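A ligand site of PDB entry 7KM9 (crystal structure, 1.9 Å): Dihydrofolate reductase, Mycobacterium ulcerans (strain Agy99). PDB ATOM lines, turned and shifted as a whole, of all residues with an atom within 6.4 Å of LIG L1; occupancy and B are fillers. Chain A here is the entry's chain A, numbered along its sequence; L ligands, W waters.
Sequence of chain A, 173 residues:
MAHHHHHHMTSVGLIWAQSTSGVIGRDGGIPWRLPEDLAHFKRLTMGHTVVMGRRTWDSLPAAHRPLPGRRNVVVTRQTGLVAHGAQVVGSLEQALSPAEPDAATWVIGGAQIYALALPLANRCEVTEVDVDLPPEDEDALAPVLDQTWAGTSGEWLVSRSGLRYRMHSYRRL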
ATOM      1  N   ILE A  15      -7.918  28.718   0.873  1.00  0.00           N
ATOM      2  CA  ILE A  15      -8.638  29.768   0.169  1.00  0.00           C
ATOM      3  C   ILE A  15      -9.737  30.284   1.092  1.00  0.00           C
ATOM      4  O   ILE A  15     -10.465  29.493   1.697  1.00  0.00           O
ATOM      5  CB  ILE A  15      -9.218  29.273  -1.171  1.00  0.00           C
ATOM      6  CG1 ILE A  15      -9.955  30.401  -1.892  1.00  0.00           C
ATOM      7  CG2 ILE A  15     -10.143  28.017  -0.998  1.00  0.00           C
ATOM      8  CD1 ILE A  15     -10.312  30.000  -3.333  1.00  0.00           C
ATOM      9  N   TRP A  16      -9.826  31.604   1.238  1.00  0.00           N
ATOM     10  CA  TRP A  16     -10.867  32.142   2.108  1.00  0.00           C
ATOM     11  C   TRP A  16     -11.185  33.570   1.679  1.00  0.00           C
ATOM     12  O   TRP A  16     -10.406  34.228   0.989  1.00  0.00           O
ATOM     13  CB  TRP A  16     -10.463  32.095   3.591  1.00  0.00           C
ATOM     14  CG  TRP A  16      -9.412  33.086   4.058  1.00  0.00           C
ATOM     15  CD1 TRP A  16      -9.606  34.417   4.413  1.00  0.00           C
ATOM     16  CD2 TRP A  16      -8.027  32.808   4.322  1.00  0.00           C
ATOM     17  NE1 TRP A  16      -8.418  34.968   4.838  1.00  0.00           N
ATOM     18  CE2 TRP A  16      -7.438  34.009   4.793  1.00  0.00           C
ATOM     19  CE3 TRP A  16      -7.228  31.673   4.200  1.00  0.00           C
ATOM     20  CZ2 TRP A  16      -6.081  34.105   5.123  1.00  0.00           C
ATOM     21  CZ3 TRP A  16      -5.888  31.756   4.521  1.00  0.00           C
ATOM     22  CH2 TRP A  16      -5.322  32.972   4.992  1.00  0.00           C
ATOM     23  N   ALA A  17     -12.360  34.037   2.094  1.00  0.00           N
ATOM     24  CA  ALA A  17     -12.736  35.444   1.941  1.00  0.00           C
ATOM     25  C   ALA A  17     -12.891  36.042   3.322  1.00  0.00           C
ATOM     26  O   ALA A  17     -13.527  35.437   4.194  1.00  0.00           O
ATOM     27  CB  ALA A  17     -14.058  35.565   1.151  1.00  0.00           C
ATOM     28  N   ILE A  30     -21.753  33.366   5.988  1.00  0.00           N
ATOM     29  CA  ILE A  30     -20.770  34.382   5.600  1.00  0.00           C
ATOM     30  C   ILE A  30     -21.494  35.723   5.592  1.00  0.00           C
ATOM     31  O   ILE A  30     -22.588  35.822   5.023  1.00  0.00           O
ATOM     32  CB  ILE A  30     -20.132  34.087   4.229  1.00  0.00           C
ATOM     33  CG1 ILE A  30     -19.419  32.732   4.306  1.00  0.00           C
ATOM     34  CG2 ILE A  30     -19.151  35.193   3.833  1.00  0.00           C
ATOM     35  CD1 ILE A  30     -18.855  32.245   2.959  1.00  0.00           C
ATOM     36  N   ASP A  37     -16.427  36.862  -5.792  1.00  0.00           N
ATOM     37  CA  ASP A  37     -15.649  35.942  -4.974  1.00  0.00           C
ATOM     38  C   ASP A  37     -16.095  34.509  -5.189  1.00  0.00           C
ATOM     39  O   ASP A  37     -15.262  33.584  -5.194  1.00  0.00           O
ATOM     40  CB  ASP A  37     -15.789  36.278  -3.484  1.00  0.00           C
ATOM     41  CG  ASP A  37     -15.107  35.236  -2.609  1.00  0.00           C
ATOM     42  OD1 ASP A  37     -13.860  35.131  -2.679  1.00  0.00           O
ATOM     43  OD2 ASP A  37     -15.811  34.484  -1.904  1.00  0.00           O
ATOM     44  N   LEU A  38     -17.389  34.291  -5.363  1.00  0.00           N
ATOM     45  CA  LEU A  38     -17.861  32.935  -5.631  1.00  0.00           C
ATOM     46  C   LEU A  38     -17.318  32.429  -6.969  1.00  0.00           C
ATOM     47  O   LEU A  38     -16.925  31.267  -7.079  1.00  0.00           O
ATOM     48  CB  LEU A  38     -19.384  32.888  -5.586  1.00  0.00           C
ATOM     49  CG  LEU A  38     -19.972  32.598  -4.183  1.00  0.00           C
ATOM     50  CD1 LEU A  38     -19.517  33.613  -3.100  1.00  0.00           C
ATOM     51  CD2 LEU A  38     -21.484  32.540  -4.229  1.00  0.00           C
ATOM     52  N   ALA A  39     -17.276  33.301  -7.984  1.00  0.00           N
ATOM     53  CA  ALA A  39     -16.676  32.909  -9.260  1.00  0.00           C
ATOM     54  C   ALA A  39     -15.182  32.602  -9.112  1.00  0.00           C
ATOM     55  O   ALA A  39     -14.671  31.641  -9.698  1.00  0.00           O
ATOM     56  CB  ALA A  39     -16.887  34.012 -10.294  1.00  0.00           C
ATOM     57  N   HIS A  40     -14.474  33.433  -8.347  1.00  0.00           N
ATOM     58  CA  HIS A  40     -13.066  33.203  -8.046  1.00  0.00           C
ATOM     59  C   HIS A  40     -12.859  31.880  -7.303  1.00  0.00           C
ATOM     60  O   HIS A  40     -11.990  31.072  -7.663  1.00  0.00           O
ATOM     61  CB  HIS A  40     -12.586  34.410  -7.224  1.00  0.00           C
ATOM     62  CG  HIS A  40     -11.209  34.293  -6.630  1.00  0.00           C
ATOM     63  ND1 HIS A  40     -10.062  34.466  -7.360  1.00  0.00           N
ATOM     64  CD2 HIS A  40     -10.815  34.124  -5.344  1.00  0.00           C
ATOM     65  CE1 HIS A  40      -9.011  34.369  -6.568  1.00  0.00           C
ATOM     66  NE2 HIS A  40      -9.446  34.156  -5.336  1.00  0.00           N
ATOM     67  N   PHE A  41     -13.689  31.641  -6.280  1.00  0.00           N
ATOM     68  CA  PHE A  41     -13.621  30.391  -5.511  1.00  0.00           C
ATOM     69  C   PHE A  41     -13.862  29.189  -6.411  1.00  0.00           C
ATOM     70  O   PHE A  41     -13.131  28.185  -6.331  1.00  0.00           O
ATOM     71  CB  PHE A  41     -14.639  30.421  -4.373  1.00  0.00           C
ATOM     72  CG  PHE A  41     -14.770  29.111  -3.650  1.00  0.00           C
ATOM     73  CD1 PHE A  41     -13.912  28.798  -2.598  1.00  0.00           C
ATOM     74  CD2 PHE A  41     -15.748  28.183  -4.016  1.00  0.00           C
ATOM     75  CE1 PHE A  41     -14.008  27.581  -1.928  1.00  0.00           C
ATOM     76  CE2 PHE A  41     -15.853  26.964  -3.349  1.00  0.00           C
ATOM     77  CZ  PHE A  41     -14.985  26.666  -2.299  1.00  0.00           C
ATOM     78  N   LYS A  42     -14.905  29.246  -7.240  1.00  0.00           N
ATOM     79  CA  LYS A  42     -15.237  28.124  -8.098  1.00  0.00           C
ATOM     80  C   LYS A  42     -14.114  27.854  -9.083  1.00  0.00           C
ATOM     81  O   LYS A  42     -13.691  26.709  -9.288  1.00  0.00           O
ATOM     82  CB  LYS A  42     -16.573  28.393  -8.820  1.00  0.00           C
ATOM     83  CG  LYS A  42     -17.100  27.166  -9.619  1.00  0.00           C
ATOM     84  CD  LYS A  42     -18.424  27.508 -10.319  1.00  0.00           C
ATOM     85  CE  LYS A  42     -19.016  26.272 -10.983  1.00  0.00           C
ATOM     86  NZ  LYS A  42     -20.170  26.639 -11.850  1.00  0.00           N
ATOM     87  N   THR A  45     -11.038  26.175  -7.347  1.00  0.00           N
ATOM     88  CA  THR A  45     -11.198  24.871  -6.730  1.00  0.00           C
ATOM     89  C   THR A  45     -11.734  23.797  -7.669  1.00  0.00           C
ATOM     90  O   THR A  45     -11.599  22.606  -7.348  1.00  0.00           O
ATOM     91  CB  THR A  45     -12.133  24.939  -5.509  1.00  0.00           C
ATOM     92  OG1 THR A  45     -13.435  25.381  -5.907  1.00  0.00           O
ATOM     93  CG2 THR A  45     -11.573  25.843  -4.399  1.00  0.00           C
ATOM     94  N   MET A  46     -12.313  24.162  -8.814  1.00  0.00           N
ATOM     95  CA  MET A  46     -12.963  23.175  -9.682  1.00  0.00           C
ATOM     96  C   MET A  46     -11.974  22.081 -10.102  1.00  0.00           C
ATOM     97  O   MET A  46     -10.833  22.355 -10.482  1.00  0.00           O
ATOM     98  CB  MET A  46     -13.549  23.853 -10.924  1.00  0.00           C
ATOM     99  CG  MET A  46     -14.272  22.880 -11.862  1.00  0.00           C
ATOM    100  SD  MET A  46     -15.676  22.104 -11.035  1.00  0.00           S
ATOM    101  CE  MET A  46     -16.599  23.572 -10.544  1.00  0.00           C
ATOM    102  N   THR A  56     -18.591  24.026   8.249  1.00  0.00           N
ATOM    103  CA  THR A  56     -18.595  24.651   6.921  1.00  0.00           C
ATOM    104  C   THR A  56     -19.424  23.828   5.938  1.00  0.00           C
ATOM    105  O   THR A  56     -20.168  24.398   5.121  1.00  0.00           O
ATOM    106  CB  THR A  56     -17.148  24.837   6.433  1.00  0.00           C
ATOM    107  OG1 THR A  56     -16.490  25.861   7.196  1.00  0.00           O
ATOM    108  CG2 THR A  56     -17.114  25.246   4.939  1.00  0.00           C
ATOM    109  N   SER A  59     -22.805  24.716   6.492  1.00  0.00           N
ATOM    110  CA  SER A  59     -23.084  26.074   6.044  1.00  0.00           C
ATOM    111  C   SER A  59     -23.307  26.179   4.534  1.00  0.00           C
ATOM    112  O   SER A  59     -23.766  27.219   4.075  1.00  0.00           O
ATOM    113  CB  SER A  59     -21.954  27.017   6.456  1.00  0.00           C
ATOM    114  OG  SER A  59     -20.842  26.913   5.582  1.00  0.00           O
ATOM    115  N   LEU A  60     -22.988  25.139   3.763  1.00  0.00           N
ATOM    116  CA  LEU A  60     -23.187  25.228   2.320  1.00  0.00           C
ATOM    117  C   LEU A  60     -24.673  25.284   2.016  1.00  0.00           C
ATOM    118  O   LEU A  60     -25.431  24.460   2.532  1.00  0.00           O
ATOM    119  CB  LEU A  60     -22.561  24.040   1.595  1.00  0.00           C
ATOM    120  CG  LEU A  60     -21.054  23.869   1.702  1.00  0.00           C
ATOM    121  CD1 LEU A  60     -20.660  22.495   1.150  1.00  0.00           C
ATOM    122  CD2 LEU A  60     -20.366  24.959   0.919  1.00  0.00           C
ATOM    123  N   PRO A  61     -25.141  26.242   1.209  1.00  0.00           N
ATOM    124  CA  PRO A  61     -26.544  26.204   0.767  1.00  0.00           C
ATOM    125  C   PRO A  61     -26.830  24.871   0.091  1.00  0.00           C
ATOM    126  O   PRO A  61     -26.002  24.330  -0.649  1.00  0.00           O
ATOM    127  CB  PRO A  61     -26.639  27.370  -0.232  1.00  0.00           C
ATOM    128  CG  PRO A  61     -25.501  28.273   0.112  1.00  0.00           C
ATOM    129  CD  PRO A  61     -24.392  27.350   0.584  1.00  0.00           C
ATOM    130  N   HIS A  64     -25.913  23.820  -3.393  1.00  0.00           N
ATOM    131  CA  HIS A  64     -24.480  23.726  -3.642  1.00  0.00           C
ATOM    132  C   HIS A  64     -23.797  22.726  -2.727  1.00  0.00           C
ATOM    133  O   HIS A  64     -22.594  22.829  -2.480  1.00  0.00           O
ATOM    134  CB  HIS A  64     -23.844  25.113  -3.495  1.00  0.00           C
ATOM    135  CG  HIS A  64     -24.609  26.185  -4.203  1.00  0.00           C
ATOM    136  ND1 HIS A  64     -24.649  26.273  -5.580  1.00  0.00           N
ATOM    137  CD2 HIS A  64     -25.404  27.175  -3.738  1.00  0.00           C
ATOM    138  CE1 HIS A  64     -25.412  27.302  -5.926  1.00  0.00           C
ATOM    139  NE2 HIS A  64     -25.881  27.854  -4.828  1.00  0.00           N
ATOM    140  N   LEU A  67     -20.334  20.392  -3.157  1.00  0.00           N
ATOM    141  CA  LEU A  67     -19.871  21.313  -4.204  1.00  0.00           C
ATOM    142  C   LEU A  67     -19.614  20.549  -5.491  1.00  0.00           C
ATOM    143  O   LEU A  67     -18.795  19.602  -5.509  1.00  0.00           O
ATOM    144  CB  LEU A  67     -18.613  22.052  -3.728  1.00  0.00           C
ATOM    145  CG  LEU A  67     -18.884  23.129  -2.673  1.00  0.00           C
ATOM    146  CD1 LEU A  67     -17.566  23.585  -2.017  1.00  0.00           C
ATOM    147  CD2 LEU A  67     -19.620  24.298  -3.322  1.00  0.00           C
ATOM    148  N   PRO A  68     -20.281  20.896  -6.589  1.00  0.00           N
ATOM    149  CA  PRO A  68     -20.201  20.080  -7.801  1.00  0.00           C
ATOM    150  C   PRO A  68     -18.825  20.140  -8.460  1.00  0.00           C
ATOM    151  O   PRO A  68     -18.113  21.136  -8.384  1.00  0.00           O
ATOM    152  CB  PRO A  68     -21.290  20.675  -8.713  1.00  0.00           C
ATOM    153  CG  PRO A  68     -21.470  22.082  -8.213  1.00  0.00           C
ATOM    154  CD  PRO A  68     -21.215  22.040  -6.735  1.00  0.00           C
ATOM    155  N   ARG A  70     -16.092  18.633  -7.683  1.00  0.00           N
ATOM    156  CA  ARG A  70     -14.968  18.559  -6.772  1.00  0.00           C
ATOM    157  C   ARG A  70     -15.213  17.415  -5.790  1.00  0.00           C
ATOM    158  O   ARG A  70     -16.343  17.197  -5.374  1.00  0.00           O
ATOM    159  CB  ARG A  70     -14.777  19.879  -5.972  1.00  0.00           C
ATOM    160  CG  ARG A  70     -14.188  21.024  -6.771  1.00  0.00           C
ATOM    161  CD  ARG A  70     -14.784  22.373  -6.340  1.00  0.00           C
ATOM    162  NE  ARG A  70     -16.170  22.504  -6.786  1.00  0.00           N
ATOM    163  CZ  ARG A  70     -16.868  23.637  -6.738  1.00  0.00           C
ATOM    164  NH1 ARG A  70     -16.354  24.748  -6.224  1.00  0.00           N
ATOM    165  NH2 ARG A  70     -18.109  23.654  -7.214  1.00  0.00           N
ATOM    166  N   VAL A 107      -8.140  23.671   0.975  1.00  0.00           N
ATOM    167  CA  VAL A 107      -8.823  23.700   2.259  1.00  0.00           C
ATOM    168  C   VAL A 107      -9.697  24.952   2.263  1.00  0.00           C
ATOM    169  O   VAL A 107      -9.191  26.070   2.132  1.00  0.00           O
ATOM    170  CB  VAL A 107      -7.822  23.727   3.422  1.00  0.00           C
ATOM    171  CG1 VAL A 107      -8.541  24.064   4.700  1.00  0.00           C
ATOM    172  CG2 VAL A 107      -7.090  22.374   3.539  1.00  0.00           C
ATOM    173  N   ILE A 108     -11.003  24.760   2.397  1.00  0.00           N
ATOM    174  CA  ILE A 108     -11.963  25.823   2.145  1.00  0.00           C
ATOM    175  C   ILE A 108     -12.660  26.286   3.424  1.00  0.00           C
ATOM    176  O   ILE A 108     -13.685  26.966   3.355  1.00  0.00           O
ATOM    177  CB  ILE A 108     -12.980  25.396   1.060  1.00  0.00           C
ATOM    178  CG1 ILE A 108     -13.899  24.258   1.538  1.00  0.00           C
ATOM    179  CG2 ILE A 108     -12.217  24.906  -0.179  1.00  0.00           C
ATOM    180  CD1 ILE A 108     -15.203  24.082   0.677  1.00  0.00           C
ATOM    181  N   GLY A 109     -12.108  25.971   4.593  1.00  0.00           N
ATOM    182  CA  GLY A 109     -12.598  26.479   5.869  1.00  0.00           C
ATOM    183  C   GLY A 109     -13.254  25.401   6.710  1.00  0.00           C
ATOM    184  O   GLY A 109     -13.335  24.230   6.334  1.00  0.00           O
ATOM    185  N   TYR A 114      -8.769  25.811   8.978  1.00  0.00           N
ATOM    186  CA  TYR A 114      -7.646  26.626   8.524  1.00  0.00           C
ATOM    187  C   TYR A 114      -6.493  26.547   9.508  1.00  0.00           C
ATOM    188  O   TYR A 114      -5.333  26.420   9.104  1.00  0.00           O
ATOM    189  CB  TYR A 114      -8.046  28.100   8.347  1.00  0.00           C
ATOM    190  CG  TYR A 114      -8.976  28.406   7.194  1.00  0.00           C
ATOM    191  CD1 TYR A 114      -8.773  27.857   5.934  1.00  0.00           C
ATOM    192  CD2 TYR A 114     -10.067  29.247   7.372  1.00  0.00           C
ATOM    193  CE1 TYR A 114      -9.633  28.128   4.875  1.00  0.00           C
ATOM    194  CE2 TYR A 114     -10.934  29.533   6.328  1.00  0.00           C
ATOM    195  CZ  TYR A 114     -10.713  28.974   5.081  1.00  0.00           C
ATOM    196  OH  TYR A 114     -11.583  29.243   4.052  1.00  0.00           O
ATOM    197  N   GLU A 125      -4.959  31.908  -0.898  1.00  0.00           N
ATOM    198  CA  GLU A 125      -5.648  32.795  -1.839  1.00  0.00           C
ATOM    199  C   GLU A 125      -6.742  33.485  -1.043  1.00  0.00           C
ATOM    200  O   GLU A 125      -7.684  32.830  -0.564  1.00  0.00           O
ATOM    201  CB  GLU A 125      -6.227  32.030  -3.020  1.00  0.00           C
ATOM    202  CG  GLU A 125      -5.156  31.317  -3.864  1.00  0.00           C
ATOM    203  CD  GLU A 125      -4.279  32.309  -4.625  1.00  0.00           C
ATOM    204  OE1 GLU A 125      -4.780  33.390  -4.979  1.00  0.00           O
ATOM    205  OE2 GLU A 125      -3.077  32.015  -4.852  1.00  0.00           O
ATOM    206  N   VAL A 126      -6.623  34.800  -0.876  1.00  0.00           N
ATOM    207  CA  VAL A 126      -7.467  35.539   0.041  1.00  0.00           C
ATOM    208  C   VAL A 126      -8.254  36.576  -0.743  1.00  0.00           C
ATOM    209  O   VAL A 126      -7.682  37.317  -1.555  1.00  0.00           O
ATOM    210  CB  VAL A 126      -6.620  36.211   1.135  1.00  0.00           C
ATOM    211  CG1 VAL A 126      -7.526  37.022   2.109  1.00  0.00           C
ATOM    212  CG2 VAL A 126      -5.760  35.154   1.841  1.00  0.00           C
ATOM    213  N   THR A 127      -9.566  36.622  -0.514  1.00  0.00           N
ATOM    214  CA  THR A 127     -10.380  37.739  -0.971  1.00  0.00           C
ATOM    215  C   THR A 127     -10.607  38.640   0.225  1.00  0.00           C
ATOM    216  O   THR A 127     -11.135  38.190   1.245  1.00  0.00           O
ATOM    217  CB  THR A 127     -11.711  37.278  -1.554  1.00  0.00           C
ATOM    218  OG1 THR A 127     -11.493  36.340  -2.612  1.00  0.00           O
ATOM    219  CG2 THR A 127     -12.511  38.494  -2.068  1.00  0.00           C
HETATM  220  C1  LIG L   1     -17.679  31.139  -1.491  1.00  0.00           C
HETATM  221  C2  LIG L   1     -17.205  31.720  -0.135  1.00  0.00           C
HETATM  222  C3  LIG L   1     -15.737  31.451  -0.056  1.00  0.00           C
HETATM  223  C4  LIG L   1     -13.640  31.999  -0.742  1.00  0.00           C
HETATM  224  C5  LIG L   1     -13.846  30.218   0.681  1.00  0.00           C
HETATM  225  C6  LIG L   1     -15.244  30.414   0.681  1.00  0.00           C
HETATM  226  C7  LIG L   1     -16.316  28.231   0.970  1.00  0.00           C
HETATM  227  C8  LIG L   1     -17.508  27.716   1.772  1.00  0.00           C
HETATM  228  C9  LIG L   1     -18.827  28.183   1.158  1.00  0.00           C
HETATM  229  C10 LIG L   1     -19.778  28.180  -1.117  1.00  0.00           C
HETATM  230  C11 LIG L   1     -21.051  28.562  -0.719  1.00  0.00           C
HETATM  231  C12 LIG L   1     -21.956  28.998  -1.690  1.00  0.00           C
HETATM  232  C13 LIG L   1     -21.601  29.060  -3.026  1.00  0.00           C
HETATM  233  C14 LIG L   1     -20.328  28.679  -3.425  1.00  0.00           C
HETATM  234  C15 LIG L   1     -19.931  28.765  -4.896  1.00  0.00           C
HETATM  235  C16 LIG L   1     -20.588  27.700  -5.798  1.00  0.00           C
HETATM  236  C17 LIG L   1     -21.235  28.324  -7.023  1.00  0.00           C
HETATM  237  C18 LIG L   1     -19.537  26.637  -6.289  1.00  0.00           C
HETATM  238  C19 LIG L   1     -19.417  28.237  -2.466  1.00  0.00           C
HETATM  239  F1  LIG L   1     -22.247  29.173  -6.608  1.00  0.00           F
HETATM  240  F2  LIG L   1     -20.342  29.132  -7.742  1.00  0.00           F
HETATM  241  N1  LIG L   1     -14.948  32.243  -0.777  1.00  0.00           N
HETATM  242  N2  LIG L   1     -12.827  32.776  -1.463  1.00  0.00           N
HETATM  243  N3  LIG L   1     -13.054  31.013  -0.049  1.00  0.00           N
HETATM  244  N4  LIG L   1     -13.280  29.228   1.401  1.00  0.00           N
HETATM  245  O1  LIG L   1     -16.048  29.601   1.456  1.00  0.00           O
HETATM  246  O2  LIG L   1     -18.817  27.738  -0.212  1.00  0.00           O
HETATM  247  O3  LIG L   1     -20.019  25.740  -7.031  1.00  0.00           O
HETATM  248  O4  LIG L   1     -18.371  26.829  -5.882  1.00  0.00           O
HETATM  249  P1  LG2 L   2     -15.218  24.648  10.835  1.00  0.00           P
HETATM  250  O1  LG2 L   2     -13.733  24.782  10.860  1.00  0.00           O
HETATM  251  O2  LG2 L   2     -15.757  24.746   9.380  1.00  0.00           O
HETATM  252  O3  LG2 L   2     -15.731  23.241  11.470  1.00  0.00           O
HETATM  253  C1  LG2 L   2     -15.559  22.953  12.869  1.00  0.00           C
HETATM  254  C2  LG2 L   2     -15.742  21.477  13.065  1.00  0.00           C
HETATM  255  O4  LG2 L   2     -14.656  20.741  12.471  1.00  0.00           O
HETATM  256  C3  LG2 L   2     -15.784  21.017  14.514  1.00  0.00           C
HETATM  257  O5  LG2 L   2     -17.031  21.337  15.118  1.00  0.00           O
HETATM  258  C4  LG2 L   2     -15.515  19.530  14.294  1.00  0.00           C
HETATM  259  O6  LG2 L   2     -16.655  18.817  13.772  1.00  0.00           O
HETATM  260  C5  LG2 L   2     -14.453  19.542  13.197  1.00  0.00           C
HETATM  261  N1  LG2 L   2     -13.086  19.500  13.719  1.00  0.00           N
HETATM  262  C6  LG2 L   2     -12.359  20.550  14.233  1.00  0.00           C
HETATM  263  N2  LG2 L   2     -11.154  20.217  14.615  1.00  0.00           N
HETATM  264  C7  LG2 L   2     -11.077  18.864  14.330  1.00  0.00           C
HETATM  265  C8  LG2 L   2     -10.049  17.917  14.515  1.00  0.00           C
HETATM  266  N3  LG2 L   2      -8.850  18.201  15.034  1.00  0.00           N
HETATM  267  N4  LG2 L   2     -10.299  16.642  14.151  1.00  0.00           N
HETATM  268  C9  LG2 L   2     -11.493  16.353  13.619  1.00  0.00           C
HETATM  269  N5  LG2 L   2     -12.538  17.156  13.394  1.00  0.00           N
HETATM  270  C10 LG2 L   2     -12.259  18.410  13.779  1.00  0.00           C
HETATM  271  O7  LG2 L   2     -15.952  25.673  11.798  1.00  0.00           O
HETATM  272  P2  LG2 L   2     -15.905  27.233  12.089  1.00  0.00           P
HETATM  273  O8  LG2 L   2     -14.509  27.572  12.473  1.00  0.00           O
HETATM  274  O9  LG2 L   2     -17.013  27.564  13.002  1.00  0.00           O
HETATM  275  O10 LG2 L   2     -16.159  27.822  10.634  1.00  0.00           O
HETATM  276  C11 LG2 L   2     -17.513  27.911  10.112  1.00  0.00           C
HETATM  277  C12 LG2 L   2     -17.868  29.348   9.854  1.00  0.00           C
HETATM  278  O11 LG2 L   2     -16.958  29.908   8.882  1.00  0.00           O
HETATM  279  C13 LG2 L   2     -19.263  29.555   9.269  1.00  0.00           C
HETATM  280  O12 LG2 L   2     -19.760  30.847   9.626  1.00  0.00           O
HETATM  281  C14 LG2 L   2     -18.977  29.521   7.774  1.00  0.00           C
HETATM  282  O13 LG2 L   2     -20.020  30.138   7.029  1.00  0.00           O
HETATM  283  C15 LG2 L   2     -17.677  30.317   7.751  1.00  0.00           C
HETATM  284  N6  LG2 L   2     -16.803  30.088   6.504  1.00  0.00           N
HETATM  285  C16 LG2 L   2     -16.358  31.183   5.868  1.00  0.00           C
HETATM  286  C17 LG2 L   2     -15.439  31.065   4.845  1.00  0.00           C
HETATM  287  C18 LG2 L   2     -14.954  32.273   4.099  1.00  0.00           C
HETATM  288  O14 LG2 L   2     -14.063  32.140   3.263  1.00  0.00           O
HETATM  289  N7  LG2 L   2     -15.489  33.466   4.394  1.00  0.00           N
HETATM  290  C19 LG2 L   2     -15.006  29.792   4.479  1.00  0.00           C
HETATM  291  C20 LG2 L   2     -15.498  28.677   5.138  1.00  0.00           C
HETATM  292  C21 LG2 L   2     -16.410  28.844   6.149  1.00  0.00           C
HETATM  293  P3  LG2 L   2     -17.743  18.114  14.703  1.00  0.00           P
HETATM  294  O15 LG2 L   2     -18.742  17.445  13.803  1.00  0.00           O
HETATM  295  O16 LG2 L   2     -16.979  17.107  15.571  1.00  0.00           O
HETATM  296  O17 LG2 L   2     -18.327  19.186  15.549  1.00  0.00           O
HETATM  297  O   HOH W   1     -22.450  25.056  -7.191  1.00  0.00           O
HETATM  298  O   HOH W   2     -19.670  31.575  -9.594  1.00  0.00           O
HETATM  299  O   HOH W   3      -9.868  33.858  -2.299  1.00  0.00           O
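Trp 16 touches LIG L1. Ala 17 touches LIG L1. Ile 30 touches LIG L1. Leu 38 touches LIG L1. CD1 of Phe 41 touches N3 of LIG L1 (3.5 Å). Lys 42 touches LIG L1 (CD to F2, 3.6 Å). CD2 of Leu 60 touches O2 of LIG L1, at 3.4 Å. Pro 61 touches LIG L1. CE1 of His 64 touches F1 of LIG L1 (3.7 Å). CD2 of Leu 67 touches C18 of LIG L1 (3.8 Å). Pro 68 touches LIG L1 (CD to O3, 3.9 Å). Thr 127 touches LIG L1 (OG1 to N2, 3.98 Å). Hydrophobic or aromatic side chains that line LIG L1: Ile 15, Ala 17, Ile 30, Leu 38, Phe 41, Leu 60, Pro 61, His 64, Leu 67, Pro 68 and Ile 108. Of the 27 residues printed, 17 come within 4 Å of LIG L1.
A nitrogen (N4) of LIG L1 sits at hydrogen-bond distance from the side-chain hydroxyl (OH) of Tyr 114 (3.1 Å). O of Ala 17 is in hydrogen-bond range of N7 of LG2 L2 (2.8 Å). N of Ala 17 sits at hydrogen-bond distance from O14 of LG2 L2 (2.8 Å). N of Thr 56 lies within hydrogen-bond range of O2 of LG2 L2, at 3.1 Å. O2 of LG2 L2 sits at hydrogen-bond distance from OG1 of Thr 56, at 2.6 Å. The backbone carbonyl oxygen of Ile 108 is in hydrogen-bond range of a nitrogen (N4) of LIG L1, at 3.0 Å. N1 of LIG L1 is in hydrogen-bond range of OD2 of Asp 37 (2.7 Å). N4 of LIG L1 is in hydrogen-bond range of O of Ile 15, 2.8 Å away. An oxygen (O3) of LIG L1 lies within salt-bridge range of the guanidinium group (NH2) of Arg 70.
Water W1 lies within hydrogen-bond range of an oxygen (O3) of LIG L1 (2.5 Å) and a ring nitrogen (ND1) of His 64 (3.0 Å). Water W3 lies within hydrogen-bond range of O of Glu 125 (3.0 Å), OG1 of Thr 127 (3.0 Å), NE2 of His 40 (3.1 Å), N2 of LIG L1 (3.3 Å) and O of Trp 16 (3.4 Å).
The side-chain hydroxyl (OH) of Tyr 114 lies close to the backbone NH (N) of Gly 109, at 3.4 Å. N of Ile 15 is in hydrogen-bond range of O of Val 107 (3.2 Å). The backbone carbonyl oxygen (O) of Phe 41 lies within hydrogen-bond range of the side-chain hydroxyl (OG1) of Thr 45. The backbone carbonyl oxygen of Trp 16 sits at hydrogen-bond distance from the backbone NH of Thr 127. The side-chain hydroxyl of Tyr 114 lies within hydrogen-bond range of the backbone carbonyl oxygen of Ile 108. The side-chain hydroxyl of Thr 127 is in hydrogen-bond range of the side-chain carboxylate of Asp 37 (2.7 Å). The side-chain hydroxyl of Tyr 114 is in hydrogen-bond range of the backbone carbonyl oxygen of Ile 15, at 2.6 Å. O of Pro 68 is in hydrogen-bond range of NH2 of Arg 70, at 2.8 Å.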
